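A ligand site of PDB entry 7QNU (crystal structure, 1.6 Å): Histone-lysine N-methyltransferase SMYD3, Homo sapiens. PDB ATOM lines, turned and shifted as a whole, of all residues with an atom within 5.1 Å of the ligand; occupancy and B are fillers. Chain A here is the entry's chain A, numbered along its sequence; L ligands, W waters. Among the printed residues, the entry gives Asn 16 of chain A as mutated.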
ATOM      1  N   ASN A  16       1.474  17.675  12.726  1.00  0.00           N
ATOM      2  CA  ASN A  16       1.101  18.280  14.003  1.00  0.00           C
ATOM      3  C   ASN A  16      -0.159  17.697  14.628  1.00  0.00           C
ATOM      4  O   ASN A  16      -0.769  18.351  15.481  1.00  0.00           O
ATOM      5  CB  ASN A  16       0.897  19.797  13.861  1.00  0.00           C
ATOM      6  CG  ASN A  16      -0.172  20.160  12.852  1.00  0.00           C
ATOM      7  OD1 ASN A  16      -1.349  19.872  13.043  1.00  0.00           O
ATOM      8  ND2 ASN A  16       0.236  20.799  11.777  1.00  0.00           N
ATOM      9  N   ARG A  17      -0.567  16.499  14.246  1.00  0.00           N
ATOM     10  CA  ARG A  17      -1.706  15.841  14.875  1.00  0.00           C
ATOM     11  C   ARG A  17      -1.418  14.363  15.099  1.00  0.00           C
ATOM     12  O   ARG A  17      -2.283  13.501  14.877  1.00  0.00           O
ATOM     13  CB  ARG A  17      -2.981  16.027  14.046  1.00  0.00           C
ATOM     14  CG  ARG A  17      -2.815  15.813  12.549  1.00  0.00           C
ATOM     15  CD  ARG A  17      -3.819  16.677  11.771  1.00  0.00           C
ATOM     16  NE  ARG A  17      -3.578  18.094  11.989  1.00  0.00           N
ATOM     17  CZ  ARG A  17      -4.297  19.079  11.449  1.00  0.00           C
ATOM     18  NH1 ARG A  17      -4.025  20.351  11.699  1.00  0.00           N
ATOM     19  NH2 ARG A  17      -5.303  18.776  10.646  1.00  0.00           N
ATOM     20  N   GLY A  18      -0.192  14.050  15.516  1.00  0.00           N
ATOM     21  CA  GLY A  18       0.166  12.682  15.812  1.00  0.00           C
ATOM     22  C   GLY A  18       0.061  11.787  14.594  1.00  0.00           C
ATOM     23  O   GLY A  18       0.350  12.186  13.462  1.00  0.00           O
ATOM     24  N   ASN A  19      -0.373  10.558  14.826  1.00  0.00           N
ATOM     25  CA  ASN A  19      -0.530   9.624  13.729  1.00  0.00           C
ATOM     26  C   ASN A  19      -1.854   9.856  13.024  1.00  0.00           C
ATOM     27  O   ASN A  19      -2.818  10.402  13.596  1.00  0.00           O
ATOM     28  CB  ASN A  19      -0.427   8.176  14.239  1.00  0.00           C
ATOM     29  CG  ASN A  19       0.919   7.862  14.846  1.00  0.00           C
ATOM     30  OD1 ASN A  19       1.947   8.158  14.237  1.00  0.00           O
ATOM     31  ND2 ASN A  19       0.928   7.291  16.028  1.00  0.00           N
ATOM     32  N   TYR A 127      -3.453  -0.488  14.016  1.00  0.00           N
ATOM     33  CA  TYR A 127      -3.216   0.392  15.166  1.00  0.00           C
ATOM     34  C   TYR A 127      -3.925  -0.272  16.340  1.00  0.00           C
ATOM     35  O   TYR A 127      -5.082  -0.685  16.197  1.00  0.00           O
ATOM     36  CB  TYR A 127      -3.722   1.788  14.809  1.00  0.00           C
ATOM     37  CG  TYR A 127      -3.170   2.937  15.622  1.00  0.00           C
ATOM     38  CD1 TYR A 127      -1.827   3.319  15.480  1.00  0.00           C
ATOM     39  CD2 TYR A 127      -3.999   3.759  16.370  1.00  0.00           C
ATOM     40  CE1 TYR A 127      -1.329   4.398  16.144  1.00  0.00           C
ATOM     41  CE2 TYR A 127      -3.492   4.861  17.051  1.00  0.00           C
ATOM     42  CZ  TYR A 127      -2.173   5.191  16.899  1.00  0.00           C
ATOM     43  OH  TYR A 127      -1.633   6.272  17.541  1.00  0.00           O
ATOM     44  N   ASP A 131      -1.520   1.406  21.151  1.00  0.00           N
ATOM     45  CA  ASP A 131      -0.998   2.512  20.379  1.00  0.00           C
ATOM     46  C   ASP A 131      -1.806   3.793  20.548  1.00  0.00           C
ATOM     47  O   ASP A 131      -1.290   4.866  20.218  1.00  0.00           O
ATOM     48  CB  ASP A 131      -0.998   2.150  18.888  1.00  0.00           C
ATOM     49  CG  ASP A 131      -0.052   1.019  18.549  1.00  0.00           C
ATOM     50  OD1 ASP A 131       1.038   0.927  19.156  1.00  0.00           O
ATOM     51  OD2 ASP A 131      -0.428   0.201  17.685  1.00  0.00           O
ATOM     52  N   LEU A 132      -3.029   3.718  21.061  1.00  0.00           N
ATOM     53  CA  LEU A 132      -3.964   4.826  20.979  1.00  0.00           C
ATOM     54  C   LEU A 132      -3.473   6.038  21.746  1.00  0.00           C
ATOM     55  O   LEU A 132      -2.824   5.922  22.798  1.00  0.00           O
ATOM     56  CB  LEU A 132      -5.325   4.416  21.527  1.00  0.00           C
ATOM     57  CG  LEU A 132      -6.068   3.307  20.808  1.00  0.00           C
ATOM     58  CD1 LEU A 132      -7.298   2.942  21.591  1.00  0.00           C
ATOM     59  CD2 LEU A 132      -6.408   3.775  19.380  1.00  0.00           C
ATOM     60  N   GLU A 133      -3.785   7.205  21.207  1.00  0.00           N
ATOM     61  CA  GLU A 133      -3.470   8.474  21.847  1.00  0.00           C
ATOM     62  C   GLU A 133      -4.178   8.579  23.195  1.00  0.00           C
ATOM     63  O   GLU A 133      -5.362   8.264  23.300  1.00  0.00           O
ATOM     64  CB  GLU A 133      -3.915   9.624  20.957  1.00  0.00           C
ATOM     65  CG  GLU A 133      -3.721  11.007  21.522  1.00  0.00           C
ATOM     66  CD  GLU A 133      -2.266  11.338  21.688  1.00  0.00           C
ATOM     67  OE1 GLU A 133      -1.617  11.651  20.664  1.00  0.00           O
ATOM     68  OE2 GLU A 133      -1.776  11.264  22.842  1.00  0.00           O
ATOM     69  N   ASN A 135      -3.365  11.629  25.225  1.00  0.00           N
ATOM     70  CA  ASN A 135      -3.349  13.074  25.502  1.00  0.00           C
ATOM     71  C   ASN A 135      -3.104  13.390  26.977  1.00  0.00           C
ATOM     72  O   ASN A 135      -3.464  14.456  27.472  1.00  0.00           O
ATOM     73  CB  ASN A 135      -4.638  13.727  25.030  1.00  0.00           C
ATOM     74  CG  ASN A 135      -4.715  13.864  23.544  1.00  0.00           C
ATOM     75  OD1 ASN A 135      -3.771  14.293  22.907  1.00  0.00           O
ATOM     76  ND2 ASN A 135      -5.858  13.508  22.993  1.00  0.00           N
ATOM     77  N   CYS A 183     -10.836   9.767  24.224  1.00  0.00           N
ATOM     78  CA  CYS A 183     -10.632  10.392  22.937  1.00  0.00           C
ATOM     79  C   CYS A 183     -10.585   9.399  21.783  1.00  0.00           C
ATOM     80  O   CYS A 183     -10.224   9.783  20.661  1.00  0.00           O
ATOM     81  CB  CYS A 183      -9.351  11.225  22.936  1.00  0.00           C
ATOM     82  SG  CYS A 183      -7.854  10.297  23.281  1.00  0.00           S
ATOM     83  N   ASN A 184     -10.929   8.128  22.021  1.00  0.00           N
ATOM     84  CA  ASN A 184     -10.987   7.125  20.955  1.00  0.00           C
ATOM     85  C   ASN A 184     -12.261   6.282  21.015  1.00  0.00           C
ATOM     86  O   ASN A 184     -12.302   5.200  20.417  1.00  0.00           O
ATOM     87  CB  ASN A 184      -9.755   6.210  21.016  1.00  0.00           C
ATOM     88  CG  ASN A 184      -8.493   6.936  20.777  1.00  0.00           C
ATOM     89  OD1 ASN A 184      -8.128   7.226  19.614  1.00  0.00           O
ATOM     90  ND2 ASN A 184      -7.801   7.280  21.865  1.00  0.00           N
ATOM     91  N   SER A 205      -9.402   4.470  14.776  1.00  0.00           N
ATOM     92  CA  SER A 205      -8.980   5.581  15.614  1.00  0.00           C
ATOM     93  C   SER A 205      -7.767   6.307  15.061  1.00  0.00           C
ATOM     94  O   SER A 205      -7.393   7.341  15.612  1.00  0.00           O
ATOM     95  CB  SER A 205      -8.656   5.112  17.031  1.00  0.00           C
ATOM     96  OG  SER A 205      -9.851   4.808  17.725  1.00  0.00           O
ATOM     97  N   LEU A 206      -7.134   5.771  14.011  1.00  0.00           N
ATOM     98  CA  LEU A 206      -6.105   6.553  13.325  1.00  0.00           C
ATOM     99  C   LEU A 206      -6.662   7.777  12.634  1.00  0.00           C
ATOM    100  O   LEU A 206      -5.906   8.701  12.345  1.00  0.00           O
ATOM    101  CB  LEU A 206      -5.383   5.663  12.298  1.00  0.00           C
ATOM    102  CG  LEU A 206      -4.216   4.827  12.826  1.00  0.00           C
ATOM    103  CD1 LEU A 206      -3.739   3.858  11.735  1.00  0.00           C
ATOM    104  CD2 LEU A 206      -3.093   5.710  13.302  1.00  0.00           C
ATOM    105  N   LEU A 207      -7.961   7.806  12.339  1.00  0.00           N
ATOM    106  CA  LEU A 207      -8.517   8.943  11.612  1.00  0.00           C
ATOM    107  C   LEU A 207      -8.577  10.181  12.481  1.00  0.00           C
ATOM    108  O   LEU A 207      -9.205  10.185  13.542  1.00  0.00           O
ATOM    109  CB  LEU A 207      -9.922   8.605  11.119  1.00  0.00           C
ATOM    110  CG  LEU A 207     -10.016   7.581   9.972  1.00  0.00           C
ATOM    111  CD1 LEU A 207     -11.352   6.890  10.055  1.00  0.00           C
ATOM    112  CD2 LEU A 207      -9.855   8.306   8.643  1.00  0.00           C
ATOM    113  N   ASN A 208      -7.950  11.256  12.022  1.00  0.00           N
ATOM    114  CA  ASN A 208      -8.051  12.543  12.673  1.00  0.00           C
ATOM    115  C   ASN A 208      -9.362  13.213  12.292  1.00  0.00           C
ATOM    116  O   ASN A 208     -10.099  12.770  11.393  1.00  0.00           O
ATOM    117  CB  ASN A 208      -6.853  13.399  12.314  1.00  0.00           C
ATOM    118  CG  ASN A 208      -5.618  13.009  13.111  1.00  0.00           C
ATOM    119  OD1 ASN A 208      -5.676  12.846  14.332  1.00  0.00           O
ATOM    120  ND2 ASN A 208      -4.504  12.844  12.415  1.00  0.00           N
ATOM    121  N   HIS A 209      -9.656  14.281  12.997  1.00  0.00           N
ATOM    122  CA  HIS A 209     -10.936  14.954  12.872  1.00  0.00           C
ATOM    123  C   HIS A 209     -10.842  16.122  11.905  1.00  0.00           C
ATOM    124  O   HIS A 209      -9.822  16.824  11.836  1.00  0.00           O
ATOM    125  CB  HIS A 209     -11.417  15.491  14.235  1.00  0.00           C
ATOM    126  CG  HIS A 209     -12.466  16.552  14.110  1.00  0.00           C
ATOM    127  ND1 HIS A 209     -13.812  16.262  14.143  1.00  0.00           N
ATOM    128  CD2 HIS A 209     -12.363  17.899  13.927  1.00  0.00           C
ATOM    129  CE1 HIS A 209     -14.501  17.386  14.002  1.00  0.00           C
ATOM    130  NE2 HIS A 209     -13.641  18.383  13.846  1.00  0.00           N
ATOM    131  N   SER A 210     -11.929  16.335  11.176  1.00  0.00           N
ATOM    132  CA  SER A 210     -12.189  17.552  10.446  1.00  0.00           C
ATOM    133  C   SER A 210     -13.662  17.882  10.545  1.00  0.00           C
ATOM    134  O   SER A 210     -14.497  16.975  10.505  1.00  0.00           O
ATOM    135  CB  SER A 210     -11.784  17.465   8.963  1.00  0.00           C
ATOM    136  OG  SER A 210     -12.139  18.657   8.312  1.00  0.00           O
ATOM    137  N   TYR A 242     -15.703  13.972  14.098  1.00  0.00           N
ATOM    138  CA  TYR A 242     -15.984  13.347  15.369  1.00  0.00           C
ATOM    139  C   TYR A 242     -17.314  13.764  15.944  1.00  0.00           C
ATOM    140  O   TYR A 242     -17.778  13.121  16.896  1.00  0.00           O
ATOM    141  CB  TYR A 242     -14.904  13.691  16.415  1.00  0.00           C
ATOM    142  CG  TYR A 242     -13.500  13.176  16.156  1.00  0.00           C
ATOM    143  CD1 TYR A 242     -13.210  12.404  15.046  1.00  0.00           C
ATOM    144  CD2 TYR A 242     -12.480  13.470  17.040  1.00  0.00           C
ATOM    145  CE1 TYR A 242     -11.934  11.952  14.812  1.00  0.00           C
ATOM    146  CE2 TYR A 242     -11.197  13.033  16.812  1.00  0.00           C
ATOM    147  CZ  TYR A 242     -10.932  12.259  15.701  1.00  0.00           C
ATOM    148  OH  TYR A 242      -9.657  11.845  15.512  1.00  0.00           O
ATOM    149  N   GLN A 259     -12.843  16.916  25.180  1.00  0.00           N
ATOM    150  CA  GLN A 259     -12.788  15.480  24.975  1.00  0.00           C
ATOM    151  C   GLN A 259     -11.554  15.031  24.219  1.00  0.00           C
ATOM    152  O   GLN A 259     -11.060  13.925  24.461  1.00  0.00           O
ATOM    153  CB  GLN A 259     -14.032  15.012  24.212  1.00  0.00           C
ATOM    154  CG  GLN A 259     -14.061  13.511  23.961  1.00  0.00           C
ATOM    155  CD  GLN A 259     -15.413  13.009  23.525  1.00  0.00           C
ATOM    156  OE1 GLN A 259     -16.374  13.793  23.396  1.00  0.00           O
ATOM    157  NE2 GLN A 259     -15.503  11.697  23.307  1.00  0.00           N
ATOM    158  N   TYR A 260     -11.066  15.862  23.287  1.00  0.00           N
ATOM    159  CA  TYR A 260     -10.005  15.440  22.388  1.00  0.00           C
ATOM    160  C   TYR A 260      -8.740  16.271  22.491  1.00  0.00           C
ATOM    161  O   TYR A 260      -7.749  15.948  21.815  1.00  0.00           O
ATOM    162  CB  TYR A 260     -10.506  15.482  20.941  1.00  0.00           C
ATOM    163  CG  TYR A 260     -11.642  14.503  20.678  1.00  0.00           C
ATOM    164  CD1 TYR A 260     -11.394  13.162  20.489  1.00  0.00           C
ATOM    165  CD2 TYR A 260     -12.950  14.931  20.646  1.00  0.00           C
ATOM    166  CE1 TYR A 260     -12.419  12.271  20.232  1.00  0.00           C
ATOM    167  CE2 TYR A 260     -13.992  14.052  20.393  1.00  0.00           C
ATOM    168  CZ  TYR A 260     -13.712  12.713  20.193  1.00  0.00           C
ATOM    169  OH  TYR A 260     -14.725  11.818  19.972  1.00  0.00           O
ATOM    170  N   CYS A 261      -8.724  17.287  23.346  1.00  0.00           N
ATOM    171  CA  CYS A 261      -7.527  18.051  23.628  1.00  0.00           C
ATOM    172  C   CYS A 261      -6.839  18.559  22.357  1.00  0.00           C
ATOM    173  O   CYS A 261      -5.611  18.462  22.195  1.00  0.00           O
ATOM    174  CB  CYS A 261      -6.532  17.225  24.461  1.00  0.00           C
ATOM    175  SG  CYS A 261      -7.083  16.689  26.052  1.00  0.00           S
ATOM    176  N   PHE A 262      -7.615  19.157  21.459  1.00  0.00           N
ATOM    177  CA  PHE A 262      -6.989  19.890  20.364  1.00  0.00           C
ATOM    178  C   PHE A 262      -7.849  21.079  19.975  1.00  0.00           C
ATOM    179  O   PHE A 262      -9.047  21.157  20.267  1.00  0.00           O
ATOM    180  CB  PHE A 262      -6.681  18.980  19.170  1.00  0.00           C
ATOM    181  CG  PHE A 262      -7.886  18.619  18.357  1.00  0.00           C
ATOM    182  CD1 PHE A 262      -8.617  17.483  18.647  1.00  0.00           C
ATOM    183  CD2 PHE A 262      -8.278  19.407  17.274  1.00  0.00           C
ATOM    184  CE1 PHE A 262      -9.756  17.136  17.876  1.00  0.00           C
ATOM    185  CE2 PHE A 262      -9.389  19.070  16.515  1.00  0.00           C
ATOM    186  CZ  PHE A 262     -10.130  17.950  16.832  1.00  0.00           C
ATOM    187  N   GLU A 263      -7.179  22.042  19.362  1.00  0.00           N
ATOM    188  CA  GLU A 263      -7.785  23.274  18.882  1.00  0.00           C
ATOM    189  C   GLU A 263      -7.976  23.103  17.379  1.00  0.00           C
ATOM    190  O   GLU A 263      -7.004  22.996  16.645  1.00  0.00           O
ATOM    191  CB  GLU A 263      -6.872  24.464  19.170  1.00  0.00           C
ATOM    192  CG  GLU A 263      -6.304  24.525  20.580  1.00  0.00           C
ATOM    193  CD  GLU A 263      -7.360  24.602  21.660  1.00  0.00           C
ATOM    194  OE1 GLU A 263      -8.491  24.999  21.335  1.00  0.00           O
ATOM    195  OE2 GLU A 263      -7.024  24.341  22.845  1.00  0.00           O
ATOM    196  N   CYS A 264      -9.217  23.064  16.923  1.00  0.00           N
ATOM    197  CA  CYS A 264      -9.454  22.760  15.517  1.00  0.00           C
ATOM    198  C   CYS A 264      -9.095  23.952  14.629  1.00  0.00           C
ATOM    199  O   CYS A 264      -9.575  25.070  14.844  1.00  0.00           O
ATOM    200  CB  CYS A 264     -10.891  22.341  15.275  1.00  0.00           C
ATOM    201  SG  CYS A 264     -11.044  21.769  13.557  1.00  0.00           S
HETATM  202  N1  LIG L   1      -3.858  11.503  16.056  1.00  0.00           N
HETATM  203  C1  LIG L   1      -4.327  10.321  16.787  1.00  0.00           C
HETATM  204  C2  LIG L   1      -3.182   9.356  17.085  1.00  0.00           C
HETATM  205  O1  LIG L   1      -3.424   8.233  17.545  1.00  0.00           O
HETATM  206  O2  LIG L   1      -1.980   9.682  16.905  1.00  0.00           O
HETATM  207  C3  LIG L   1      -5.418   9.593  15.998  1.00  0.00           C
HETATM  208  C4  LIG L   1      -6.807  10.210  16.155  1.00  0.00           C
HETATM  209  S1  LIG L   1      -7.459   9.847  17.801  1.00  0.00           S
HETATM  210  C5  LIG L   1      -9.074   9.203  17.350  1.00  0.00           C
HETATM  211  C6  LIG L   1      -8.016  11.509  18.325  1.00  0.00           C
HETATM  212  C7  LIG L   1      -6.859  12.393  18.773  1.00  0.00           C
HETATM  213  O3  LIG L   1      -6.033  12.836  17.662  1.00  0.00           O
HETATM  214  C8  LIG L   1      -7.377  13.686  19.487  1.00  0.00           C
HETATM  215  O4  LIG L   1      -7.603  13.503  20.829  1.00  0.00           O
HETATM  216  C9  LIG L   1      -6.256  14.666  19.176  1.00  0.00           C
HETATM  217  O5  LIG L   1      -5.243  14.459  20.115  1.00  0.00           O
HETATM  218  C10 LIG L   1      -5.778  14.234  17.784  1.00  0.00           C
HETATM  219  N2  LIG L   1      -6.487  14.935  16.715  1.00  0.00           N
HETATM  220  C11 LIG L   1      -7.581  14.448  16.040  1.00  0.00           C
HETATM  221  N3  LIG L   1      -7.951  15.377  15.153  1.00  0.00           N
HETATM  222  C12 LIG L   1      -7.130  16.478  15.263  1.00  0.00           C
HETATM  223  C13 LIG L   1      -7.090  17.671  14.576  1.00  0.00           C
HETATM  224  N4  LIG L   1      -7.949  17.954  13.621  1.00  0.00           N
HETATM  225  N5  LIG L   1      -6.117  18.598  14.909  1.00  0.00           N
HETATM  226  C14 LIG L   1      -5.212  18.299  15.890  1.00  0.00           C
HETATM  227  N6  LIG L   1      -5.251  17.105  16.560  1.00  0.00           N
HETATM  228  C15 LIG L   1      -6.219  16.194  16.249  1.00  0.00           C
HETATM  229  O   HOH W   1      -5.447   7.216  19.098  1.00  0.00           O
HETATM  230  O   HOH W   2      -4.318  16.622  21.139  1.00  0.00           O
HETATM  231  O   HOH W   3      -2.810  20.466  15.044  1.00  0.00           O
HETATM  232  O   HOH W   4     -10.958   8.146  14.745  1.00  0.00           O
HETATM  233  O   HOH W   5      -8.513  20.428  12.180  1.00  0.00           O
HETATM  234  O   HOH W   6      -2.739  12.726  18.261  1.00  0.00           O
HETATM  235  O   HOH W   7      -0.252   9.488  18.841  1.00  0.00           O
HETATM  236  O   HOH W   8      -3.295  17.215  18.530  1.00  0.00           O
HETATM  237  O   HOH W   9      -6.135  21.307  14.469  1.00  0.00           O
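OH of Tyr 127 sits at hydrogen-bond distance from O1 of the ligand (2.7 Å). The side-chain amide nitrogen (ND2) of Asn 135 sits at hydrogen-bond distance from an oxygen (O4) of the ligand. O2 of the ligand is in hydrogen-bond range of N of Asn 19, 2.8 Å away. The backbone NH (N) of His 209 lies within hydrogen-bond range of a nitrogen (N3) of the ligand (3.0 Å). An oxygen (O4) of the ligand is in hydrogen-bond range of the backbone carbonyl oxygen (O) of Tyr 260, 2.6 Å away. The backbone carbonyl oxygen (O) of Arg 17 is in hydrogen-bond range of a nitrogen (N1) of the ligand (2.8 Å). The side-chain amide oxygen of Asn 208 sits at hydrogen-bond distance from a nitrogen (N1) of the ligand (2.8 Å). A nitrogen (N1) of the ligand is in hydrogen-bond range of the backbone carbonyl oxygen of Asn 19 (2.9 Å). O of His 209 is in hydrogen-bond range of N4 of the ligand, 2.8 Å away.
O of Tyr 260 lies within hydrogen-bond range of ND2 of Asn 135. OD1 of Asn 16 lies within hydrogen-bond range of NH1 of Arg 17 (3.0 Å). The backbone carbonyl oxygen (O) of Glu 133 is in hydrogen-bond range of the side-chain amide nitrogen (ND2) of Asn 184, 3.0 Å away. The side-chain amide nitrogen (ND2) of Asn 135 lies within hydrogen-bond range of the side-chain sulfur (SG) of Cys 183. ND2 of Asn 19 lies within hydrogen-bond range of OH of Tyr 127 (3.1 Å). A ring nitrogen (ND1) of His 209 sits at hydrogen-bond distance from the backbone NH (N) of Tyr 242, 3.0 Å away. O of Arg 17 is in hydrogen-bond range of ND2 of Asn 208 (3.4 Å). O of Glu 133 is in hydrogen-bond range of SG of Cys 183, at 3.2 Å.
A sulfur (S1) of the ligand lies close to the side-chain amide oxygen of Asn 184, at 3.3 Å. S1 of the ligand sits close to O of Ser 205 (3.3 Å). The side-chain hydroxyl (OH) of Tyr 242 lies close to a sulfur (S1) of the ligand (3.8 Å). Merely in contact with the ligand: Phe 262, Leu 207, Cys 183, Glu 133, Gly 18 and Leu 206. Hydrophobic or aromatic side chains within 4 Å of the ligand: Tyr 127, His 209, Tyr 242, Tyr 260 and Phe 262. 16 residues have an atom within 4 Å of the ligand: Arg 17, Gly 18, Asn 19, Tyr 127, Glu 133, Asn 135, Cys 183, Asn 184, Ser 205, Leu 206, Leu 207, Asn 208, His 209, Tyr 242, Tyr 260 and Phe 262.
Water W2 lies within hydrogen-bond range of the backbone carbonyl oxygen of Cys 261, an oxygen (O5) of the ligand and the side-chain amide oxygen of Asn 135. Water W7 lies within hydrogen-bond range of an oxygen (O2) of the ligand (2.6 Å) and the side-chain carboxylate of Glu 133 (3.1 Å). Water W9 lies within hydrogen-bond range of a nitrogen (N5) of the ligand (2.7 Å) and the backbone carbonyl oxygen (O) of Glu 263 (2.9 Å). Water W1 lies within hydrogen-bond range of N of Glu 133 (2.7 Å), OD1 of Asn 184 (2.7 Å) and O1 of the ligand (2.7 Å). Water W6 bridges N1 of the ligand (2.8 Å) and OE1 of Glu 133 (2.9 Å).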
